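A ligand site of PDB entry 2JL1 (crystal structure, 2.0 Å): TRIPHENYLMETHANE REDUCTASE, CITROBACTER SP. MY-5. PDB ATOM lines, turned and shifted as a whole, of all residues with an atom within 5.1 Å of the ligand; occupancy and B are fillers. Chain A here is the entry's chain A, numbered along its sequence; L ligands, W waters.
The side-chain hydroxyl (OG) of Ser 74 lies within hydrogen-bond range of an oxygen (O13) of the ligand (3.0 Å). O10 of the ligand sits at hydrogen-bond distance from OH of Tyr 143. The backbone NH of Tyr 143 is in hydrogen-bond range of an oxygen (O14) of the ligand, 2.9 Å away. An oxygen (O13) of the ligand lies within hydrogen-bond range of the backbone carbonyl oxygen (O) of Gly 75, 2.5 Å away. The side-chain hydroxyl of Thr 9 is in hydrogen-bond range of an oxygen (O15) of the ligand (2.8 Å). The backbone carbonyl oxygen (O) of Ala 141 is in hydrogen-bond range of a nitrogen (N7) of the ligand (3.1 Å). An oxygen (O2) of the ligand is in hydrogen-bond range of the backbone NH of Gln 11, 2.9 Å away. An oxygen (O5) of the ligand lies within hydrogen-bond range of the backbone NH of Gly 10 (3.0 Å). N3 of the ligand sits at hydrogen-bond distance from OD1 of Asp 53 (3.1 Å). O of Ser 74 sits at hydrogen-bond distance from O12 of the ligand (2.5 Å). N of Tyr 54 is in hydrogen-bond range of N4 of the ligand, 2.9 Å away. OD1 of Asn 55 lies within hydrogen-bond range of N3 of the ligand. O16 of the ligand is in salt-bridge range of NH2 of Arg 34 (2.9 Å). An oxygen (O8) of the ligand lies within hydrogen-bond range of the backbone NH of Leu 12 (2.6 Å). The guanidinium group of Arg 175 lies within salt-bridge range of an oxygen (O9) of the ligand (2.7 Å).
The side-chain amide oxygen (OD1) of Asn 35 lies within hydrogen-bond range of the backbone NH (N) of Lys 38 (3.4 Å). The backbone carbonyl oxygen (O) of Ile 73 lies within hydrogen-bond range of the side-chain hydroxyl (OH) of Tyr 54, at 3.2 Å. OD1 of Asp 53 lies within hydrogen-bond range of N of Asn 55 (2.9 Å). The side-chain hydroxyl (OG1) of Thr 105 is in hydrogen-bond range of the backbone NH (N) of Ser 74 (2.9 Å). The side-chain amide nitrogen of Asn 55 lies close to the side-chain amide nitrogen of Gln 86, at 2.7 Å. OH of Tyr 54 sits at hydrogen-bond distance from N of Gly 7 (3.5 Å). OE1 of Gln 11 lies within hydrogen-bond range of NH1 of Arg 175 (3.4 Å).
O12 of the ligand lies close to N of Pro 76, at 3.2 Å. Merely in contact with the ligand: Gly 7, Asn 35, Lys 38, Gly 52, Ile 73, His 77 and Leu 142. Of the 28 residues printed, 21 come within 4 Å of the ligand.
Water W6 lies within hydrogen-bond range of O9 of the ligand (2.7 Å) and NH2 of Arg 175 (2.9 Å). Water W10 lies within hydrogen-bond range of the side-chain hydroxyl of Thr 9 (2.7 Å), an oxygen (O17) of the ligand (2.7 Å), the backbone NH of Asn 35 (3.0 Å) and the backbone NH of Arg 34 (3.4 Å). Water W5 bridges a nitrogen (N5) of the ligand (2.8 Å) and the backbone NH (N) of Gly 7 (3.0 Å). Water W13 lies within hydrogen-bond range of the backbone NH (N) of Gly 13, the backbone carbonyl oxygen (O) of Gly 7 and an oxygen (O8) of the ligand. Water W7 lies within hydrogen-bond range of the side-chain hydroxyl (OH) of Tyr 143 (2.7 Å), the side-chain amide nitrogen (ND2) of Asn 140 (2.9 Å) and an oxygen (O11) of the ligand (3.3 Å). Water W3 lies within hydrogen-bond range of OD1 of Asn 55, NE2 of Gln 86 and N3 of the ligand.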
ATOM      1  N   GLY A   7     -14.259  15.230   2.481  1.00  0.00           N
ATOM      2  CA  GLY A   7     -13.151  16.211   2.548  1.00  0.00           C
ATOM      3  C   GLY A   7     -13.573  17.676   2.319  1.00  0.00           C
ATOM      4  O   GLY A   7     -12.752  18.527   1.886  1.00  0.00           O
ATOM      5  N   ALA A   8     -14.825  17.984   2.635  1.00  0.00           N
ATOM      6  CA  ALA A   8     -15.442  19.270   2.266  1.00  0.00           C
ATOM      7  C   ALA A   8     -14.812  20.532   2.873  1.00  0.00           C
ATOM      8  O   ALA A   8     -14.957  21.613   2.280  1.00  0.00           O
ATOM      9  CB  ALA A   8     -16.940  19.261   2.506  1.00  0.00           C
ATOM     10  N   THR A   9     -14.149  20.409   4.015  1.00  0.00           N
ATOM     11  CA  THR A   9     -13.430  21.529   4.643  1.00  0.00           C
ATOM     12  C   THR A   9     -11.970  21.619   4.169  1.00  0.00           C
ATOM     13  O   THR A   9     -11.241  22.555   4.522  1.00  0.00           O
ATOM     14  CB  THR A   9     -13.436  21.447   6.191  1.00  0.00           C
ATOM     15  OG1 THR A   9     -12.867  20.198   6.603  1.00  0.00           O
ATOM     16  CG2 THR A   9     -14.835  21.570   6.751  1.00  0.00           C
ATOM     17  N   GLY A  10     -11.535  20.638   3.387  1.00  0.00           N
ATOM     18  CA  GLY A  10     -10.182  20.671   2.832  1.00  0.00           C
ATOM     19  C   GLY A  10     -10.118  21.619   1.651  1.00  0.00           C
ATOM     20  O   GLY A  10     -11.133  22.195   1.237  1.00  0.00           O
ATOM     21  N   GLN A  11      -8.919  21.794   1.104  1.00  0.00           N
ATOM     22  CA  GLN A  11      -8.717  22.806   0.069  1.00  0.00           C
ATOM     23  C   GLN A  11      -9.450  22.407  -1.197  1.00  0.00           C
ATOM     24  O   GLN A  11     -10.232  23.192  -1.749  1.00  0.00           O
ATOM     25  CB  GLN A  11      -7.212  23.088  -0.163  1.00  0.00           C
ATOM     26  CG  GLN A  11      -6.501  23.449   1.162  1.00  0.00           C
ATOM     27  CD  GLN A  11      -5.028  23.741   0.981  1.00  0.00           C
ATOM     28  OE1 GLN A  11      -4.667  24.822   0.508  1.00  0.00           O
ATOM     29  NE2 GLN A  11      -4.167  22.796   1.380  1.00  0.00           N
ATOM     30  N   LEU A  12      -9.265  21.171  -1.642  1.00  0.00           N
ATOM     31  CA  LEU A  12      -9.932  20.720  -2.870  1.00  0.00           C
ATOM     32  C   LEU A  12     -11.448  20.676  -2.699  1.00  0.00           C
ATOM     33  O   LEU A  12     -12.167  21.148  -3.572  1.00  0.00           O
ATOM     34  CB  LEU A  12      -9.417  19.341  -3.319  1.00  0.00           C
ATOM     35  CG  LEU A  12      -9.892  18.803  -4.671  1.00  0.00           C
ATOM     36  CD1 LEU A  12      -9.213  19.553  -5.839  1.00  0.00           C
ATOM     37  CD2 LEU A  12      -9.597  17.289  -4.778  1.00  0.00           C
ATOM     38  N   GLY A  13     -11.904  20.091  -1.605  1.00  0.00           N
ATOM     39  CA  GLY A  13     -13.333  19.946  -1.266  1.00  0.00           C
ATOM     40  C   GLY A  13     -14.086  21.256  -1.194  1.00  0.00           C
ATOM     41  O   GLY A  13     -15.203  21.370  -1.695  1.00  0.00           O
ATOM     42  N   ARG A  34     -15.216  15.701   8.802  1.00  0.00           N
ATOM     43  CA  ARG A  34     -14.828  15.089  10.083  1.00  0.00           C
ATOM     44  C   ARG A  34     -15.084  16.046  11.268  1.00  0.00           C
ATOM     45  O   ARG A  34     -15.551  15.632  12.348  1.00  0.00           O
ATOM     46  CB  ARG A  34     -13.344  14.653  10.014  1.00  0.00           C
ATOM     47  CG  ARG A  34     -12.772  14.152  11.338  1.00  0.00           C
ATOM     48  CD  ARG A  34     -11.348  13.636  11.165  1.00  0.00           C
ATOM     49  NE  ARG A  34     -10.425  14.641  10.634  1.00  0.00           N
ATOM     50  CZ  ARG A  34      -9.101  14.529  10.688  1.00  0.00           C
ATOM     51  NH1 ARG A  34      -8.547  13.467  11.266  1.00  0.00           N
ATOM     52  NH2 ARG A  34      -8.325  15.482  10.178  1.00  0.00           N
ATOM     53  N   ASN A  35     -14.821  17.330  11.056  1.00  0.00           N
ATOM     54  CA  ASN A  35     -14.882  18.353  12.109  1.00  0.00           C
ATOM     55  C   ASN A  35     -16.050  19.284  11.743  1.00  0.00           C
ATOM     56  O   ASN A  35     -15.919  20.139  10.873  1.00  0.00           O
ATOM     57  CB  ASN A  35     -13.528  19.099  12.166  1.00  0.00           C
ATOM     58  CG  ASN A  35     -13.467  20.225  13.227  1.00  0.00           C
ATOM     59  OD1 ASN A  35     -14.459  20.586  13.844  1.00  0.00           O
ATOM     60  ND2 ASN A  35     -12.270  20.768  13.419  1.00  0.00           N
ATOM     61  N   LYS A  38     -15.622  23.235  11.982  1.00  0.00           N
ATOM     62  CA  LYS A  38     -14.943  23.752  10.785  1.00  0.00           C
ATOM     63  C   LYS A  38     -15.896  24.088   9.636  1.00  0.00           C
ATOM     64  O   LYS A  38     -15.624  24.998   8.849  1.00  0.00           O
ATOM     65  CB  LYS A  38     -13.958  22.700  10.272  1.00  0.00           C
ATOM     66  CG  LYS A  38     -12.529  22.856  10.705  1.00  0.00           C
ATOM     67  CD  LYS A  38     -11.617  23.136   9.504  1.00  0.00           C
ATOM     68  CE  LYS A  38     -10.251  22.466   9.640  1.00  0.00           C
ATOM     69  NZ  LYS A  38      -9.395  22.988  10.776  1.00  0.00           N
ATOM     70  N   GLY A  52     -18.919  12.792   8.862  1.00  0.00           N
ATOM     71  CA  GLY A  52     -18.504  11.533   8.260  1.00  0.00           C
ATOM     72  C   GLY A  52     -17.023  11.430   8.482  1.00  0.00           C
ATOM     73  O   GLY A  52     -16.266  12.242   7.952  1.00  0.00           O
ATOM     74  N   ASP A  53     -16.617  10.463   9.297  1.00  0.00           N
ATOM     75  CA  ASP A  53     -15.207  10.242   9.595  1.00  0.00           C
ATOM     76  C   ASP A  53     -14.779   8.878   9.037  1.00  0.00           C
ATOM     77  O   ASP A  53     -15.384   7.860   9.402  1.00  0.00           O
ATOM     78  CB  ASP A  53     -15.012  10.305  11.115  1.00  0.00           C
ATOM     79  CG  ASP A  53     -13.545  10.229  11.533  1.00  0.00           C
ATOM     80  OD1 ASP A  53     -12.714   9.607  10.806  1.00  0.00           O
ATOM     81  OD2 ASP A  53     -13.224  10.783  12.600  1.00  0.00           O
ATOM     82  N   TYR A  54     -13.750   8.853   8.178  1.00  0.00           N
ATOM     83  CA  TYR A  54     -13.317   7.606   7.486  1.00  0.00           C
ATOM     84  C   TYR A  54     -12.847   6.521   8.462  1.00  0.00           C
ATOM     85  O   TYR A  54     -12.734   5.362   8.092  1.00  0.00           O
ATOM     86  CB  TYR A  54     -12.192   7.838   6.467  1.00  0.00           C
ATOM     87  CG  TYR A  54     -12.407   8.960   5.491  1.00  0.00           C
ATOM     88  CD1 TYR A  54     -13.692   9.390   5.142  1.00  0.00           C
ATOM     89  CD2 TYR A  54     -11.309   9.595   4.920  1.00  0.00           C
ATOM     90  CE1 TYR A  54     -13.881  10.436   4.245  1.00  0.00           C
ATOM     91  CE2 TYR A  54     -11.468  10.626   4.013  1.00  0.00           C
ATOM     92  CZ  TYR A  54     -12.749  11.050   3.688  1.00  0.00           C
ATOM     93  OH  TYR A  54     -12.888  12.077   2.790  1.00  0.00           O
ATOM     94  N   ASN A  55     -12.566   6.925   9.694  1.00  0.00           N
ATOM     95  CA  ASN A  55     -12.212   6.004  10.765  1.00  0.00           C
ATOM     96  C   ASN A  55     -13.449   5.396  11.453  1.00  0.00           C
ATOM     97  O   ASN A  55     -13.318   4.491  12.277  1.00  0.00           O
ATOM     98  CB  ASN A  55     -11.353   6.720  11.804  1.00  0.00           C
ATOM     99  CG  ASN A  55     -10.005   7.146  11.256  1.00  0.00           C
ATOM    100  OD1 ASN A  55      -9.538   8.249  11.530  1.00  0.00           O
ATOM    101  ND2 ASN A  55      -9.382   6.263  10.486  1.00  0.00           N
ATOM    102  N   ILE A  73     -13.389  12.238  -1.973  1.00  0.00           N
ATOM    103  CA  ILE A  73     -12.071  12.876  -2.095  1.00  0.00           C
ATOM    104  C   ILE A  73     -11.150  12.091  -1.200  1.00  0.00           C
ATOM    105  O   ILE A  73     -11.491  11.842  -0.050  1.00  0.00           O
ATOM    106  CB  ILE A  73     -12.118  14.387  -1.699  1.00  0.00           C
ATOM    107  CG1 ILE A  73     -12.989  15.177  -2.704  1.00  0.00           C
ATOM    108  CG2 ILE A  73     -10.672  14.964  -1.521  1.00  0.00           C
ATOM    109  CD1 ILE A  73     -13.112  16.659  -2.379  1.00  0.00           C
ATOM    110  N   SER A  74      -9.975  11.685  -1.711  1.00  0.00           N
ATOM    111  CA  SER A  74      -9.083  10.799  -0.960  1.00  0.00           C
ATOM    112  C   SER A  74      -8.611  11.435   0.353  1.00  0.00           C
ATOM    113  O   SER A  74      -8.546  12.649   0.466  1.00  0.00           O
ATOM    114  CB  SER A  74      -7.883  10.358  -1.813  1.00  0.00           C
ATOM    115  OG  SER A  74      -7.268  11.459  -2.480  1.00  0.00           O
ATOM    116  N   GLY A  75      -8.296  10.607   1.339  1.00  0.00           N
ATOM    117  CA  GLY A  75      -7.810  11.117   2.622  1.00  0.00           C
ATOM    118  C   GLY A  75      -6.395  11.671   2.543  1.00  0.00           C
ATOM    119  O   GLY A  75      -5.711  11.424   1.565  1.00  0.00           O
ATOM    120  N   PRO A  76      -5.970  12.450   3.572  1.00  0.00           N
ATOM    121  CA  PRO A  76      -4.580  12.913   3.692  1.00  0.00           C
ATOM    122  C   PRO A  76      -3.690  11.694   3.807  1.00  0.00           C
ATOM    123  O   PRO A  76      -4.105  10.682   4.342  1.00  0.00           O
ATOM    124  CB  PRO A  76      -4.576  13.689   5.000  1.00  0.00           C
ATOM    125  CG  PRO A  76      -6.007  14.125   5.195  1.00  0.00           C
ATOM    126  CD  PRO A  76      -6.806  12.951   4.680  1.00  0.00           C
ATOM    127  N   HIS A  77      -2.468  11.767   3.307  1.00  0.00           N
ATOM    128  CA  HIS A  77      -1.795  10.491   3.096  1.00  0.00           C
ATOM    129  C   HIS A  77      -0.480  10.289   3.817  1.00  0.00           C
ATOM    130  O   HIS A  77       0.564  10.022   3.194  1.00  0.00           O
ATOM    131  CB  HIS A  77      -1.681  10.201   1.601  1.00  0.00           C
ATOM    132  CG  HIS A  77      -1.134  11.328   0.799  1.00  0.00           C
ATOM    133  ND1 HIS A  77       0.216  11.575   0.714  1.00  0.00           N
ATOM    134  CD2 HIS A  77      -1.740  12.254   0.017  1.00  0.00           C
ATOM    135  CE1 HIS A  77       0.423  12.613  -0.085  1.00  0.00           C
ATOM    136  NE2 HIS A  77      -0.757  13.045  -0.511  1.00  0.00           N
ATOM    137  N   GLN A  86      -9.104   3.081   5.537  1.00  0.00           N
ATOM    138  CA  GLN A  86     -10.072   4.190   5.570  1.00  0.00           C
ATOM    139  C   GLN A  86     -10.894   4.226   4.296  1.00  0.00           C
ATOM    140  O   GLN A  86     -12.126   4.299   4.322  1.00  0.00           O
ATOM    141  CB  GLN A  86      -9.363   5.526   5.784  1.00  0.00           C
ATOM    142  CG  GLN A  86      -8.782   5.703   7.188  1.00  0.00           C
ATOM    143  CD  GLN A  86      -8.024   6.989   7.338  1.00  0.00           C
ATOM    144  OE1 GLN A  86      -7.644   7.625   6.351  1.00  0.00           O
ATOM    145  NE2 GLN A  86      -7.794   7.403   8.582  1.00  0.00           N
ATOM    146  N   THR A 105     -11.344  10.885  -6.428  1.00  0.00           N
ATOM    147  CA  THR A 105     -10.134  11.620  -6.779  1.00  0.00           C
ATOM    148  C   THR A 105      -8.927  10.708  -6.625  1.00  0.00           C
ATOM    149  O   THR A 105      -8.372  10.535  -5.511  1.00  0.00           O
ATOM    150  CB  THR A 105      -9.936  12.886  -5.899  1.00  0.00           C
ATOM    151  OG1 THR A 105      -9.856  12.497  -4.525  1.00  0.00           O
ATOM    152  CG2 THR A 105     -11.092  13.875  -6.103  1.00  0.00           C
ATOM    153  N   TYR A 107      -5.246   9.299  -8.977  1.00  0.00           N
ATOM    154  CA  TYR A 107      -3.945   9.869  -9.327  1.00  0.00           C
ATOM    155  C   TYR A 107      -3.680   9.455 -10.777  1.00  0.00           C
ATOM    156  O   TYR A 107      -3.827   8.282 -11.117  1.00  0.00           O
ATOM    157  CB  TYR A 107      -2.894   9.365  -8.345  1.00  0.00           C
ATOM    158  CG  TYR A 107      -1.478   9.862  -8.592  1.00  0.00           C
ATOM    159  CD1 TYR A 107      -1.204  11.231  -8.601  1.00  0.00           C
ATOM    160  CD2 TYR A 107      -0.434   8.955  -8.780  1.00  0.00           C
ATOM    161  CE1 TYR A 107       0.109  11.708  -8.822  1.00  0.00           C
ATOM    162  CE2 TYR A 107       0.885   9.422  -9.009  1.00  0.00           C
ATOM    163  CZ  TYR A 107       1.146  10.808  -9.024  1.00  0.00           C
ATOM    164  OH  TYR A 107       2.435  11.290  -9.244  1.00  0.00           O
ATOM    165  N   HIS A 121      -4.341   4.565  -4.493  1.00  0.00           N
ATOM    166  CA  HIS A 121      -5.367   4.998  -5.428  1.00  0.00           C
ATOM    167  C   HIS A 121      -5.869   3.851  -6.293  1.00  0.00           C
ATOM    168  O   HIS A 121      -7.080   3.714  -6.525  1.00  0.00           O
ATOM    169  CB  HIS A 121      -4.856   6.183  -6.269  1.00  0.00           C
ATOM    170  CG  HIS A 121      -4.726   7.442  -5.468  1.00  0.00           C
ATOM    171  ND1 HIS A 121      -5.781   7.997  -4.769  1.00  0.00           N
ATOM    172  CD2 HIS A 121      -3.643   8.218  -5.205  1.00  0.00           C
ATOM    173  CE1 HIS A 121      -5.353   9.064  -4.121  1.00  0.00           C
ATOM    174  NE2 HIS A 121      -4.070   9.228  -4.378  1.00  0.00           N
ATOM    175  N   ASN A 140      -6.368  12.746 -10.699  1.00  0.00           N
ATOM    176  CA  ASN A 140      -5.803  14.093 -10.670  1.00  0.00           C
ATOM    177  C   ASN A 140      -4.287  14.069 -10.816  1.00  0.00           C
ATOM    178  O   ASN A 140      -3.627  13.174 -10.326  1.00  0.00           O
ATOM    179  CB  ASN A 140      -6.179  14.813  -9.366  1.00  0.00           C
ATOM    180  CG  ASN A 140      -7.652  15.205  -9.324  1.00  0.00           C
ATOM    181  OD1 ASN A 140      -8.354  15.192 -10.344  1.00  0.00           O
ATOM    182  ND2 ASN A 140      -8.135  15.520  -8.133  1.00  0.00           N
ATOM    183  N   ALA A 141      -3.750  15.099 -11.486  1.00  0.00           N
ATOM    184  CA  ALA A 141      -2.335  15.408 -11.465  1.00  0.00           C
ATOM    185  C   ALA A 141      -1.908  15.910 -10.075  1.00  0.00           C
ATOM    186  O   ALA A 141      -2.740  16.278  -9.237  1.00  0.00           O
ATOM    187  CB  ALA A 141      -2.033  16.518 -12.488  1.00  0.00           C
ATOM    188  N   LEU A 142      -0.589  15.928  -9.837  1.00  0.00           N
ATOM    189  CA  LEU A 142      -0.045  16.723  -8.753  1.00  0.00           C
ATOM    190  C   LEU A 142      -0.578  18.163  -8.841  1.00  0.00           C
ATOM    191  O   LEU A 142      -0.809  18.660  -9.947  1.00  0.00           O
ATOM    192  CB  LEU A 142       1.475  16.732  -8.813  1.00  0.00           C
ATOM    193  CG  LEU A 142       2.165  15.368  -8.734  1.00  0.00           C
ATOM    194  CD1 LEU A 142       3.682  15.575  -9.000  1.00  0.00           C
ATOM    195  CD2 LEU A 142       1.916  14.719  -7.342  1.00  0.00           C
ATOM    196  N   TYR A 143      -0.788  18.814  -7.694  1.00  0.00           N
ATOM    197  CA  TYR A 143      -1.242  20.198  -7.652  1.00  0.00           C
ATOM    198  C   TYR A 143      -0.141  21.189  -7.996  1.00  0.00           C
ATOM    199  O   TYR A 143       0.909  21.156  -7.407  1.00  0.00           O
ATOM    200  CB  TYR A 143      -1.795  20.569  -6.255  1.00  0.00           C
ATOM    201  CG  TYR A 143      -2.916  19.702  -5.744  1.00  0.00           C
ATOM    202  CD1 TYR A 143      -3.891  19.204  -6.604  1.00  0.00           C
ATOM    203  CD2 TYR A 143      -3.039  19.420  -4.379  1.00  0.00           C
ATOM    204  CE1 TYR A 143      -4.960  18.395  -6.130  1.00  0.00           C
ATOM    205  CE2 TYR A 143      -4.093  18.617  -3.889  1.00  0.00           C
ATOM    206  CZ  TYR A 143      -5.042  18.133  -4.772  1.00  0.00           C
ATOM    207  OH  TYR A 143      -6.088  17.379  -4.313  1.00  0.00           O
ATOM    208  N   ARG A 175      -5.510  23.078  -8.028  1.00  0.00           N
ATOM    209  CA  ARG A 175      -6.670  22.526  -7.293  1.00  0.00           C
ATOM    210  C   ARG A 175      -7.943  23.117  -7.829  1.00  0.00           C
ATOM    211  O   ARG A 175      -8.952  22.413  -7.928  1.00  0.00           O
ATOM    212  CB  ARG A 175      -6.612  22.903  -5.823  1.00  0.00           C
ATOM    213  CG  ARG A 175      -5.792  22.012  -4.993  1.00  0.00           C
ATOM    214  CD  ARG A 175      -6.082  22.308  -3.534  1.00  0.00           C
ATOM    215  NE  ARG A 175      -4.980  21.775  -2.756  1.00  0.00           N
ATOM    216  CZ  ARG A 175      -3.937  22.489  -2.366  1.00  0.00           C
ATOM    217  NH1 ARG A 175      -3.895  23.788  -2.620  1.00  0.00           N
ATOM    218  NH2 ARG A 175      -2.965  21.903  -1.677  1.00  0.00           N
HETATM  219  P1  LIG L   1      -6.461  18.856   2.430  1.00  0.00           P
HETATM  220  O1  LIG L   1      -5.298  18.482   3.275  1.00  0.00           O
HETATM  221  O2  LIG L   1      -6.755  20.300   2.348  1.00  0.00           O
HETATM  222  O3  LIG L   1      -7.772  18.071   2.885  1.00  0.00           O
HETATM  223  C1  LIG L   1      -7.797  16.732   3.331  1.00  0.00           C
HETATM  224  C2  LIG L   1      -9.217  16.519   3.817  1.00  0.00           C
HETATM  225  O4  LIG L   1      -9.395  15.193   4.311  1.00  0.00           O
HETATM  226  C3  LIG L   1      -9.506  17.484   4.968  1.00  0.00           C
HETATM  227  O5  LIG L   1     -10.753  18.099   4.762  1.00  0.00           O
HETATM  228  C4  LIG L   1      -9.579  16.609   6.173  1.00  0.00           C
HETATM  229  O6  LIG L   1     -10.560  17.054   7.057  1.00  0.00           O
HETATM  230  C5  LIG L   1     -10.031  15.296   5.573  1.00  0.00           C
HETATM  231  N1  LIG L   1      -9.748  14.192   6.500  1.00  0.00           N
HETATM  232  C6  LIG L   1      -8.564  13.879   7.092  1.00  0.00           C
HETATM  233  N2  LIG L   1      -8.762  12.789   7.875  1.00  0.00           N
HETATM  234  C7  LIG L   1     -10.073  12.432   7.789  1.00  0.00           C
HETATM  235  C8  LIG L   1     -10.816  11.415   8.380  1.00  0.00           C
HETATM  236  N3  LIG L   1     -10.253  10.552   9.228  1.00  0.00           N
HETATM  237  N4  LIG L   1     -12.154  11.302   8.087  1.00  0.00           N
HETATM  238  C9  LIG L   1     -12.757  12.197   7.233  1.00  0.00           C
HETATM  239  N5  LIG L   1     -12.021  13.202   6.640  1.00  0.00           N
HETATM  240  C10 LIG L   1     -10.692  13.313   6.930  1.00  0.00           C
HETATM  241  O7  LIG L   1      -6.175  18.255   0.945  1.00  0.00           O
HETATM  242  P2  LIG L   1      -6.471  18.883  -0.506  1.00  0.00           P
HETATM  243  O8  LIG L   1      -7.871  19.339  -0.502  1.00  0.00           O
HETATM  244  O9  LIG L   1      -5.382  19.840  -0.852  1.00  0.00           O
HETATM  245  O10 LIG L   1      -6.408  17.551  -1.474  1.00  0.00           O
HETATM  246  C11 LIG L   1      -7.403  16.542  -1.346  1.00  0.00           C
HETATM  247  C12 LIG L   1      -6.848  15.113  -1.357  1.00  0.00           C
HETATM  248  O11 LIG L   1      -6.024  14.936  -2.500  1.00  0.00           O
HETATM  249  C13 LIG L   1      -5.969  14.811  -0.153  1.00  0.00           C
HETATM  250  O12 LIG L   1      -6.644  14.249   0.951  1.00  0.00           O
HETATM  251  C14 LIG L   1      -4.908  13.866  -0.687  1.00  0.00           C
HETATM  252  O13 LIG L   1      -5.245  12.496  -0.595  1.00  0.00           O
HETATM  253  C15 LIG L   1      -4.845  14.222  -2.154  1.00  0.00           C
HETATM  254  N6  LIG L   1      -3.619  14.988  -2.394  1.00  0.00           N
HETATM  255  C16 LIG L   1      -3.252  15.180  -3.691  1.00  0.00           C
HETATM  256  C17 LIG L   1      -2.097  15.839  -3.984  1.00  0.00           C
HETATM  257  C18 LIG L   1      -1.681  16.027  -5.381  1.00  0.00           C
HETATM  258  O14 LIG L   1      -0.532  16.841  -5.599  1.00  0.00           O
HETATM  259  N7  LIG L   1      -2.389  15.392  -6.323  1.00  0.00           N
HETATM  260  C19 LIG L   1      -1.327  16.409  -2.950  1.00  0.00           C
HETATM  261  C20 LIG L   1      -1.757  16.294  -1.660  1.00  0.00           C
HETATM  262  C21 LIG L   1      -2.890  15.526  -1.373  1.00  0.00           C
HETATM  263  P3  LIG L   1     -10.203  18.008   8.317  1.00  0.00           P
HETATM  264  O15 LIG L   1     -10.494  19.432   7.884  1.00  0.00           O
HETATM  265  O16 LIG L   1      -8.750  17.907   8.732  1.00  0.00           O
HETATM  266  O17 LIG L   1     -11.120  17.547   9.430  1.00  0.00           O
HETATM  267  O   HOH W   1      -6.112  16.392   7.562  1.00  0.00           O
HETATM  268  O   HOH W   2      -7.607  20.351   6.728  1.00  0.00           O
HETATM  269  O   HOH W   3      -7.207   9.758  10.469  1.00  0.00           O
HETATM  270  O   HOH W   4      -0.243  19.296  -2.019  1.00  0.00           O
HETATM  271  O   HOH W   5     -14.216  14.524   5.405  1.00  0.00           O
HETATM  272  O   HOH W   6      -2.823  19.450  -0.188  1.00  0.00           O
HETATM  273  O   HOH W   7      -6.461  15.131  -5.814  1.00  0.00           O
HETATM  274  O   HOH W   8      -7.305  22.406   4.671  1.00  0.00           O
HETATM  275  O   HOH W   9     -10.753  13.785   2.317  1.00  0.00           O
HETATM  276  O   HOH W  10     -13.517  18.583   8.607  1.00  0.00           O
HETATM  277  O   HOH W  11     -13.677  17.814   5.705  1.00  0.00           O
HETATM  278  O   HOH W  12      -3.668  12.883  -6.568  1.00  0.00           O
HETATM  279  O   HOH W  13     -10.550  18.388   0.113  1.00  0.00           O
HETATM  280  O   HOH W  14      -3.196  11.722  -4.160  1.00  0.00           O
